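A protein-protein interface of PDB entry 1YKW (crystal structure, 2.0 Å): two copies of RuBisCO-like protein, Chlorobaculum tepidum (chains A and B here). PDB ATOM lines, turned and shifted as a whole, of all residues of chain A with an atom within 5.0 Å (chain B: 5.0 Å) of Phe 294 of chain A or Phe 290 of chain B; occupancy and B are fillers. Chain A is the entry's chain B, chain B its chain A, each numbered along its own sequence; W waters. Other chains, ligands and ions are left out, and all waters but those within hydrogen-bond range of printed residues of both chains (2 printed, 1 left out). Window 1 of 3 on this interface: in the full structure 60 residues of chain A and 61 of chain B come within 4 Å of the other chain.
Among the printed residues, pairs that only touch across the chains: Cys 117 of chain A with Phe 290 of chain B (3.4 Å), Gly 118 of chain A with Pro 289 of chain B (3.7 Å), Gly 118 of chain A with Phe 290 of chain B (3.9 Å), Glu 119 of chain A with Phe 288 of chain B (3.9 Å), Tyr 122 of chain A with Ala 292 of chain B (3.7 Å), Tyr 122 of chain A with Ser 293 of chain B (3.7 Å), Phe 290 of chain A with Phe 294 of chain B (3.7 Å), Ser 293 of chain A with Phe 294 of chain B (3.4 Å), Phe 294 of chain A with Phe 290 of chain B (3.8 Å), Phe 294 of chain A with Ser 293 of chain B (3.5 Å), Phe 294 of chain A with Phe 294 of chain B (3.995 Å), Tyr 300 of chain A with Ser 293 of chain B (3.7 Å) and Ile 302 of chain A with Phe 290 of chain B (3.3 Å).
Phe 290 of chain A touches Phe 294 of chain B, and with the chains exchanged Phe 294 of chain A touches Phe 290 of chain B. Ser 293 of chain A touches Phe 294 of chain B, and with the chains exchanged Phe 294 of chain A touches Ser 293 of chain B. Phe 294 of chain A touches its own counterpart, Phe 294 of chain B. Positions printed for both chains: 266, 290, 291, 292, 293 and 294.
Of the printed residues of chain B, Glu 119 of chain A touches Phe 288. Printed residues of chain B within 4 Å of Phe 294 of chain A: Phe 290 (3.8 Å), Ser 293 (3.5 Å) and Phe 294 (3.995 Å). Of the printed residues of chain B, Tyr 300 of chain A touches Ala 292 (3.1 Å) and Ser 293 (3.7 Å). Phe 290 of chain B touches just these residues of chain A: Cys 117 (3.4 Å), Gly 118 (3.9 Å), Phe 294 (3.8 Å) and Ile 302 (3.3 Å). Printed residues of chain A within 4 Å of Ser 293 of chain B: Tyr 122, Phe 294 and Tyr 300. Of the printed residues of chain A, Phe 294 of chain B touches Phe 290 (3.7 Å), Ser 293 (3.4 Å) and Phe 294 (3.995 Å). The nearest printed residue of chain B that does not touch Phe 294 of chain A is Ala 292 of chain B (6.6 Å). The nearest residue of chain A that does not touch Phe 290 of chain B is Met 307 of chain A (4.1 Å). The nearest printed residue of chain B that does not touch Gly 118 of chain A is Phe 288 of chain B (6.0 Å).
Water W1 lies within hydrogen-bond range of the backbone carbonyl oxygen of Ser 293 of chain A (2.7 Å) and the backbone carbonyl oxygen of Ser 293 of chain B (2.9 Å). Water W2 bridges N of Phe 290 of chain B (2.9 Å) and O of Gly 118 of chain A (3.0 Å).
O of Ala 292 of chain B lies within hydrogen-bond range of OH of Tyr 300 of chain A (3.1 Å).
The side-chain hydroxyl (OG) of Ser 293 of chain B lies within hydrogen-bond range of the backbone carbonyl oxygen (O) of Phe 290 of chain B, 2.8 Å away. SG of Cys 117 of chain A sits close to O of Leu 113 of chain A (3.7 Å). The side-chain hydroxyl (OH) of Tyr 122 of chain A is in hydrogen-bond range of the backbone carbonyl oxygen (O) of Gly 301 of chain A (2.8 Å). The backbone carbonyl oxygen (O) of Phe 290 of chain A lies within hydrogen-bond range of the side-chain hydroxyl (OG) of Ser 293 of chain A, at 2.7 Å. N of Ile 302 of chain A is in hydrogen-bond range of O of Phe 294 of chain A, at 3.0 Å.
Along chain A the printed residues that touch a printed residue of chain B span positions 117 to 302. Of the 9 printed residues of chain B, 6 touch a printed residue of chain A. Hydrophobic or aromatic side chains of chain B that line the printed part of chain A: Phe 288, Pro 289, Phe 290, Ala 292 and Phe 294. Among the printed residues, no Asp or Glu carboxylate lies within 4 Å of a Lys or Arg side-chain nitrogen of the other chain.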
ATOM      1  N   LEU A 113      -8.463  10.216  19.010  1.00  0.00           N
ATOM      2  CA  LEU A 113      -9.553  10.899  18.334  1.00  0.00           C
ATOM      3  C   LEU A 113     -10.893  10.232  18.627  1.00  0.00           C
ATOM      4  O   LEU A 113     -11.896  10.923  18.914  1.00  0.00           O
ATOM      5  CB  LEU A 113      -9.321  10.971  16.796  1.00  0.00           C
ATOM      6  CG  LEU A 113      -8.094  11.801  16.367  1.00  0.00           C
ATOM      7  CD1 LEU A 113      -7.906  11.822  14.838  1.00  0.00           C
ATOM      8  CD2 LEU A 113      -8.183  13.243  16.877  1.00  0.00           C
ATOM      9  N   CYS A 117     -13.187  13.053  20.646  1.00  0.00           N
ATOM     10  CA  CYS A 117     -14.092  13.717  19.715  1.00  0.00           C
ATOM     11  C   CYS A 117     -14.846  12.682  18.884  1.00  0.00           C
ATOM     12  O   CYS A 117     -14.845  12.744  17.665  1.00  0.00           O
ATOM     13  CB  CYS A 117     -13.408  14.811  18.874  1.00  0.00           C
ATOM     14  SG  CYS A 117     -11.695  14.552  18.341  1.00  0.00           S
ATOM     15  N   GLY A 118     -15.488  11.725  19.557  1.00  0.00           N
ATOM     16  CA  GLY A 118     -16.014  10.552  18.871  1.00  0.00           C
ATOM     17  C   GLY A 118     -17.494  10.431  19.173  1.00  0.00           C
ATOM     18  O   GLY A 118     -18.161  11.449  19.329  1.00  0.00           O
ATOM     19  N   GLU A 119     -18.034   9.223  19.262  1.00  0.00           N
ATOM     20  CA  GLU A 119     -19.503   9.113  19.326  1.00  0.00           C
ATOM     21  C   GLU A 119     -20.089   9.675  20.636  1.00  0.00           C
ATOM     22  O   GLU A 119     -21.089  10.399  20.621  1.00  0.00           O
ATOM     23  CB  GLU A 119     -20.001   7.694  18.960  1.00  0.00           C
ATOM     24  CG  GLU A 119     -20.626   6.867  20.087  1.00  0.00           C
ATOM     25  CD  GLU A 119     -21.537   5.751  19.551  1.00  0.00           C
ATOM     26  OE1 GLU A 119     -22.761   5.766  19.822  1.00  0.00           O
ATOM     27  OE2 GLU A 119     -21.032   4.858  18.839  1.00  0.00           O
ATOM     28  N   TYR A 122     -20.267  13.742  20.838  1.00  0.00           N
ATOM     29  CA  TYR A 122     -21.251  14.512  20.077  1.00  0.00           C
ATOM     30  C   TYR A 122     -22.669  13.941  20.160  1.00  0.00           C
ATOM     31  O   TYR A 122     -23.623  14.596  19.738  1.00  0.00           O
ATOM     32  CB  TYR A 122     -20.792  14.663  18.614  1.00  0.00           C
ATOM     33  CG  TYR A 122     -19.509  15.461  18.491  1.00  0.00           C
ATOM     34  CD1 TYR A 122     -18.297  14.827  18.153  1.00  0.00           C
ATOM     35  CD2 TYR A 122     -19.493  16.839  18.723  1.00  0.00           C
ATOM     36  CE1 TYR A 122     -17.094  15.559  18.033  1.00  0.00           C
ATOM     37  CE2 TYR A 122     -18.284  17.579  18.624  1.00  0.00           C
ATOM     38  CZ  TYR A 122     -17.100  16.916  18.280  1.00  0.00           C
ATOM     39  OH  TYR A 122     -15.912  17.605  18.181  1.00  0.00           O
ATOM     40  N   LEU A 266      -4.873  16.515   7.302  1.00  0.00           N
ATOM     41  CA  LEU A 266      -6.155  15.882   7.572  1.00  0.00           C
ATOM     42  C   LEU A 266      -6.657  14.978   6.443  1.00  0.00           C
ATOM     43  O   LEU A 266      -7.144  13.883   6.731  1.00  0.00           O
ATOM     44  CB  LEU A 266      -7.218  16.905   7.997  1.00  0.00           C
ATOM     45  CG  LEU A 266      -7.423  16.973   9.522  1.00  0.00           C
ATOM     46  CD1 LEU A 266      -7.966  15.651  10.028  1.00  0.00           C
ATOM     47  CD2 LEU A 266      -6.197  17.370  10.326  1.00  0.00           C
ATOM     48  N   PHE A 290      -9.430  20.984   4.831  1.00  0.00           N
ATOM     49  CA  PHE A 290     -10.398  20.179   5.589  1.00  0.00           C
ATOM     50  C   PHE A 290     -10.714  20.686   7.011  1.00  0.00           C
ATOM     51  O   PHE A 290     -11.850  20.542   7.449  1.00  0.00           O
ATOM     52  CB  PHE A 290      -9.999  18.671   5.637  1.00  0.00           C
ATOM     53  CG  PHE A 290     -11.169  17.735   5.923  1.00  0.00           C
ATOM     54  CD1 PHE A 290     -12.047  17.373   4.919  1.00  0.00           C
ATOM     55  CD2 PHE A 290     -11.398  17.258   7.218  1.00  0.00           C
ATOM     56  CE1 PHE A 290     -13.145  16.527   5.181  1.00  0.00           C
ATOM     57  CE2 PHE A 290     -12.486  16.417   7.511  1.00  0.00           C
ATOM     58  CZ  PHE A 290     -13.364  16.041   6.491  1.00  0.00           C
ATOM     59  N   ILE A 291      -9.720  21.247   7.705  1.00  0.00           N
ATOM     60  CA  ILE A 291      -9.810  21.606   9.132  1.00  0.00           C
ATOM     61  C   ILE A 291     -10.973  22.589   9.370  1.00  0.00           C
ATOM     62  O   ILE A 291     -11.643  22.500  10.396  1.00  0.00           O
ATOM     63  CB  ILE A 291      -8.471  22.179   9.743  1.00  0.00           C
ATOM     64  CG1 ILE A 291      -7.332  21.140   9.812  1.00  0.00           C
ATOM     65  CG2 ILE A 291      -8.663  22.776  11.179  1.00  0.00           C
ATOM     66  CD1 ILE A 291      -5.899  21.776  10.030  1.00  0.00           C
ATOM     67  N   ALA A 292     -11.212  23.510   8.431  1.00  0.00           N
ATOM     68  CA  ALA A 292     -12.305  24.502   8.595  1.00  0.00           C
ATOM     69  C   ALA A 292     -13.679  23.862   8.700  1.00  0.00           C
ATOM     70  O   ALA A 292     -14.595  24.459   9.261  1.00  0.00           O
ATOM     71  CB  ALA A 292     -12.292  25.575   7.478  1.00  0.00           C
ATOM     72  N   SER A 293     -13.833  22.657   8.161  1.00  0.00           N
ATOM     73  CA  SER A 293     -15.160  22.022   8.133  1.00  0.00           C
ATOM     74  C   SER A 293     -15.644  21.760   9.560  1.00  0.00           C
ATOM     75  O   SER A 293     -16.840  21.792   9.794  1.00  0.00           O
ATOM     76  CB  SER A 293     -15.183  20.720   7.308  1.00  0.00           C
ATOM     77  OG  SER A 293     -14.351  19.732   7.894  1.00  0.00           O
ATOM     78  N   PHE A 294     -14.715  21.561  10.504  1.00  0.00           N
ATOM     79  CA  PHE A 294     -15.074  21.251  11.890  1.00  0.00           C
ATOM     80  C   PHE A 294     -14.593  22.309  12.911  1.00  0.00           C
ATOM     81  O   PHE A 294     -14.923  22.226  14.089  1.00  0.00           O
ATOM     82  CB  PHE A 294     -14.629  19.821  12.267  1.00  0.00           C
ATOM     83  CG  PHE A 294     -13.156  19.563  12.149  1.00  0.00           C
ATOM     84  CD1 PHE A 294     -12.237  20.175  13.031  1.00  0.00           C
ATOM     85  CD2 PHE A 294     -12.664  18.705  11.157  1.00  0.00           C
ATOM     86  CE1 PHE A 294     -10.870  19.950  12.895  1.00  0.00           C
ATOM     87  CE2 PHE A 294     -11.309  18.466  11.039  1.00  0.00           C
ATOM     88  CZ  PHE A 294     -10.401  19.071  11.895  1.00  0.00           C
ATOM     89  N   SER A 295     -13.856  23.327  12.468  1.00  0.00           N
ATOM     90  CA  SER A 295     -13.321  24.318  13.410  1.00  0.00           C
ATOM     91  C   SER A 295     -13.850  25.747  13.272  1.00  0.00           C
ATOM     92  O   SER A 295     -13.530  26.602  14.114  1.00  0.00           O
ATOM     93  CB  SER A 295     -11.788  24.327  13.366  1.00  0.00           C
ATOM     94  OG  SER A 295     -11.357  24.761  12.104  1.00  0.00           O
ATOM     95  N   ARG A 296     -14.660  26.004  12.243  1.00  0.00           N
ATOM     96  CA  ARG A 296     -15.161  27.351  12.006  1.00  0.00           C
ATOM     97  C   ARG A 296     -16.247  27.843  13.002  1.00  0.00           C
ATOM     98  O   ARG A 296     -16.259  29.018  13.352  1.00  0.00           O
ATOM     99  CB  ARG A 296     -15.650  27.538  10.558  1.00  0.00           C
ATOM    100  CG  ARG A 296     -16.314  28.910  10.374  1.00  0.00           C
ATOM    101  CD  ARG A 296     -16.236  29.461   8.974  1.00  0.00           C
ATOM    102  NE  ARG A 296     -14.850  29.564   8.561  1.00  0.00           N
ATOM    103  CZ  ARG A 296     -14.471  29.606   7.286  1.00  0.00           C
ATOM    104  NH1 ARG A 296     -15.400  29.632   6.320  1.00  0.00           N
ATOM    105  NH2 ARG A 296     -13.164  29.628   6.991  1.00  0.00           N
ATOM    106  N   TYR A 300     -19.145  25.050  18.181  1.00  0.00           N
ATOM    107  CA  TYR A 300     -19.325  23.646  17.851  1.00  0.00           C
ATOM    108  C   TYR A 300     -18.106  23.054  17.149  1.00  0.00           C
ATOM    109  O   TYR A 300     -17.542  23.717  16.273  1.00  0.00           O
ATOM    110  CB  TYR A 300     -20.578  23.470  16.975  1.00  0.00           C
ATOM    111  CG  TYR A 300     -20.932  22.012  16.854  1.00  0.00           C
ATOM    112  CD1 TYR A 300     -21.783  21.403  17.774  1.00  0.00           C
ATOM    113  CD2 TYR A 300     -20.367  21.228  15.844  1.00  0.00           C
ATOM    114  CE1 TYR A 300     -22.077  20.042  17.669  1.00  0.00           C
ATOM    115  CE2 TYR A 300     -20.625  19.888  15.740  1.00  0.00           C
ATOM    116  CZ  TYR A 300     -21.476  19.302  16.654  1.00  0.00           C
ATOM    117  OH  TYR A 300     -21.739  17.960  16.535  1.00  0.00           O
ATOM    118  N   GLY A 301     -17.711  21.817  17.490  1.00  0.00           N
ATOM    119  CA  GLY A 301     -16.697  21.081  16.716  1.00  0.00           C
ATOM    120  C   GLY A 301     -15.373  20.833  17.445  1.00  0.00           C
ATOM    121  O   GLY A 301     -15.356  20.287  18.552  1.00  0.00           O
ATOM    122  N   ILE A 302     -14.261  21.237  16.832  1.00  0.00           N
ATOM    123  CA  ILE A 302     -12.914  21.137  17.427  1.00  0.00           C
ATOM    124  C   ILE A 302     -12.153  22.423  17.172  1.00  0.00           C
ATOM    125  O   ILE A 302     -12.092  22.878  16.016  1.00  0.00           O
ATOM    126  CB  ILE A 302     -12.138  19.938  16.814  1.00  0.00           C
ATOM    127  CG1 ILE A 302     -13.022  18.695  16.814  1.00  0.00           C
ATOM    128  CG2 ILE A 302     -10.828  19.684  17.572  1.00  0.00           C
ATOM    129  CD1 ILE A 302     -12.442  17.542  16.062  1.00  0.00           C
ATOM    130  N   MET A 307      -5.883  20.749  16.472  1.00  0.00           N
ATOM    131  CA  MET A 307      -5.341  20.104  15.279  1.00  0.00           C
ATOM    132  C   MET A 307      -3.870  20.492  15.079  1.00  0.00           C
ATOM    133  O   MET A 307      -3.083  19.651  14.663  1.00  0.00           O
ATOM    134  CB  MET A 307      -6.160  20.382  14.008  1.00  0.00           C
ATOM    135  CG  MET A 307      -7.520  19.682  14.046  1.00  0.00           C
ATOM    136  SD  MET A 307      -7.322  17.875  14.003  1.00  0.00           S
ATOM    137  CE  MET A 307      -8.696  17.321  14.971  1.00  0.00           C
ATOM    138  N   LEU B 266     -13.099   7.652  10.026  1.00  0.00           N
ATOM    139  CA  LEU B 266     -12.480   8.967  10.001  1.00  0.00           C
ATOM    140  C   LEU B 266     -11.240   9.101  10.866  1.00  0.00           C
ATOM    141  O   LEU B 266     -10.235   9.646  10.373  1.00  0.00           O
ATOM    142  CB  LEU B 266     -13.496  10.082  10.296  1.00  0.00           C
ATOM    143  CG  LEU B 266     -14.112  10.729   9.050  1.00  0.00           C
ATOM    144  CD1 LEU B 266     -13.075  11.588   8.283  1.00  0.00           C
ATOM    145  CD2 LEU B 266     -14.841   9.771   8.129  1.00  0.00           C
ATOM    146  N   PRO B 267     -11.294   8.628  12.143  1.00  0.00           N
ATOM    147  CA  PRO B 267     -10.066   8.618  12.937  1.00  0.00           C
ATOM    148  C   PRO B 267      -8.869   7.951  12.256  1.00  0.00           C
ATOM    149  O   PRO B 267      -7.781   8.496  12.403  1.00  0.00           O
ATOM    150  CB  PRO B 267     -10.482   7.843  14.211  1.00  0.00           C
ATOM    151  CG  PRO B 267     -11.909   8.320  14.394  1.00  0.00           C
ATOM    152  CD  PRO B 267     -12.430   8.153  12.960  1.00  0.00           C
ATOM    153  N   PHE B 288     -18.867   5.362  13.072  1.00  0.00           N
ATOM    154  CA  PHE B 288     -18.972   6.793  12.767  1.00  0.00           C
ATOM    155  C   PHE B 288     -18.312   7.894  13.649  1.00  0.00           C
ATOM    156  O   PHE B 288     -18.628   9.074  13.448  1.00  0.00           O
ATOM    157  CB  PHE B 288     -20.448   7.168  12.543  1.00  0.00           C
ATOM    158  CG  PHE B 288     -21.327   6.940  13.736  1.00  0.00           C
ATOM    159  CD1 PHE B 288     -21.589   7.987  14.640  1.00  0.00           C
ATOM    160  CD2 PHE B 288     -21.954   5.707  13.935  1.00  0.00           C
ATOM    161  CE1 PHE B 288     -22.435   7.799  15.720  1.00  0.00           C
ATOM    162  CE2 PHE B 288     -22.815   5.503  15.017  1.00  0.00           C
ATOM    163  CZ  PHE B 288     -23.060   6.565  15.926  1.00  0.00           C
ATOM    164  N   PRO B 289     -17.403   7.557  14.591  1.00  0.00           N
ATOM    165  CA  PRO B 289     -16.815   8.655  15.386  1.00  0.00           C
ATOM    166  C   PRO B 289     -16.201   9.765  14.529  1.00  0.00           C
ATOM    167  O   PRO B 289     -15.628   9.487  13.453  1.00  0.00           O
ATOM    168  CB  PRO B 289     -15.717   7.946  16.207  1.00  0.00           C
ATOM    169  CG  PRO B 289     -16.319   6.556  16.413  1.00  0.00           C
ATOM    170  CD  PRO B 289     -16.869   6.252  15.018  1.00  0.00           C
ATOM    171  N   PHE B 290     -16.346  10.991  15.006  1.00  0.00           N
ATOM    172  CA  PHE B 290     -15.702  12.193  14.450  1.00  0.00           C
ATOM    173  C   PHE B 290     -16.590  12.892  13.399  1.00  0.00           C
ATOM    174  O   PHE B 290     -16.532  14.102  13.316  1.00  0.00           O
ATOM    175  CB  PHE B 290     -14.299  11.883  13.877  1.00  0.00           C
ATOM    176  CG  PHE B 290     -13.432  13.115  13.637  1.00  0.00           C
ATOM    177  CD1 PHE B 290     -12.629  13.613  14.644  1.00  0.00           C
ATOM    178  CD2 PHE B 290     -13.409  13.745  12.385  1.00  0.00           C
ATOM    179  CE1 PHE B 290     -11.817  14.742  14.428  1.00  0.00           C
ATOM    180  CE2 PHE B 290     -12.635  14.885  12.155  1.00  0.00           C
ATOM    181  CZ  PHE B 290     -11.822  15.383  13.168  1.00  0.00           C
ATOM    182  N   ILE B 291     -17.385  12.126  12.634  1.00  0.00           N
ATOM    183  CA  ILE B 291     -18.132  12.624  11.472  1.00  0.00           C
ATOM    184  C   ILE B 291     -19.012  13.813  11.914  1.00  0.00           C
ATOM    185  O   ILE B 291     -19.118  14.796  11.189  1.00  0.00           O
ATOM    186  CB  ILE B 291     -18.998  11.534  10.730  1.00  0.00           C
ATOM    187  CG1 ILE B 291     -18.129  10.497   9.983  1.00  0.00           C
ATOM    188  CG2 ILE B 291     -19.948  12.184   9.703  1.00  0.00           C
ATOM    189  CD1 ILE B 291     -18.908   9.257   9.466  1.00  0.00           C
ATOM    190  N   ALA B 292     -19.570  13.746  13.123  1.00  0.00           N
ATOM    191  CA  ALA B 292     -20.492  14.803  13.600  1.00  0.00           C
ATOM    192  C   ALA B 292     -19.850  16.157  13.758  1.00  0.00           C
ATOM    193  O   ALA B 292     -20.542  17.176  13.779  1.00  0.00           O
ATOM    194  CB  ALA B 292     -21.208  14.387  14.921  1.00  0.00           C
ATOM    195  N   SER B 293     -18.528  16.192  13.907  1.00  0.00           N
ATOM    196  CA  SER B 293     -17.887  17.489  14.158  1.00  0.00           C
ATOM    197  C   SER B 293     -18.037  18.392  12.924  1.00  0.00           C
ATOM    198  O   SER B 293     -18.046  19.606  13.063  1.00  0.00           O
ATOM    199  CB  SER B 293     -16.418  17.332  14.544  1.00  0.00           C
ATOM    200  OG  SER B 293     -15.695  16.743  13.483  1.00  0.00           O
ATOM    201  N   PHE B 294     -18.166  17.801  11.734  1.00  0.00           N
ATOM    202  CA  PHE B 294     -18.305  18.614  10.510  1.00  0.00           C
ATOM    203  C   PHE B 294     -19.668  18.530   9.793  1.00  0.00           C
ATOM    204  O   PHE B 294     -19.919  19.282   8.851  1.00  0.00           O
ATOM    205  CB  PHE B 294     -17.152  18.376   9.527  1.00  0.00           C
ATOM    206  CG  PHE B 294     -16.941  16.933   9.128  1.00  0.00           C
ATOM    207  CD1 PHE B 294     -17.840  16.281   8.267  1.00  0.00           C
ATOM    208  CD2 PHE B 294     -15.856  16.234   9.599  1.00  0.00           C
ATOM    209  CE1 PHE B 294     -17.658  14.962   7.913  1.00  0.00           C
ATOM    210  CE2 PHE B 294     -15.624  14.892   9.226  1.00  0.00           C
ATOM    211  CZ  PHE B 294     -16.521  14.248   8.385  1.00  0.00           C
HETATM  212  O   HOH W   1     -18.775  22.013  11.682  1.00  0.00           O
HETATM  213  O   HOH W   2     -18.788  11.608  16.418  1.00  0.00           O
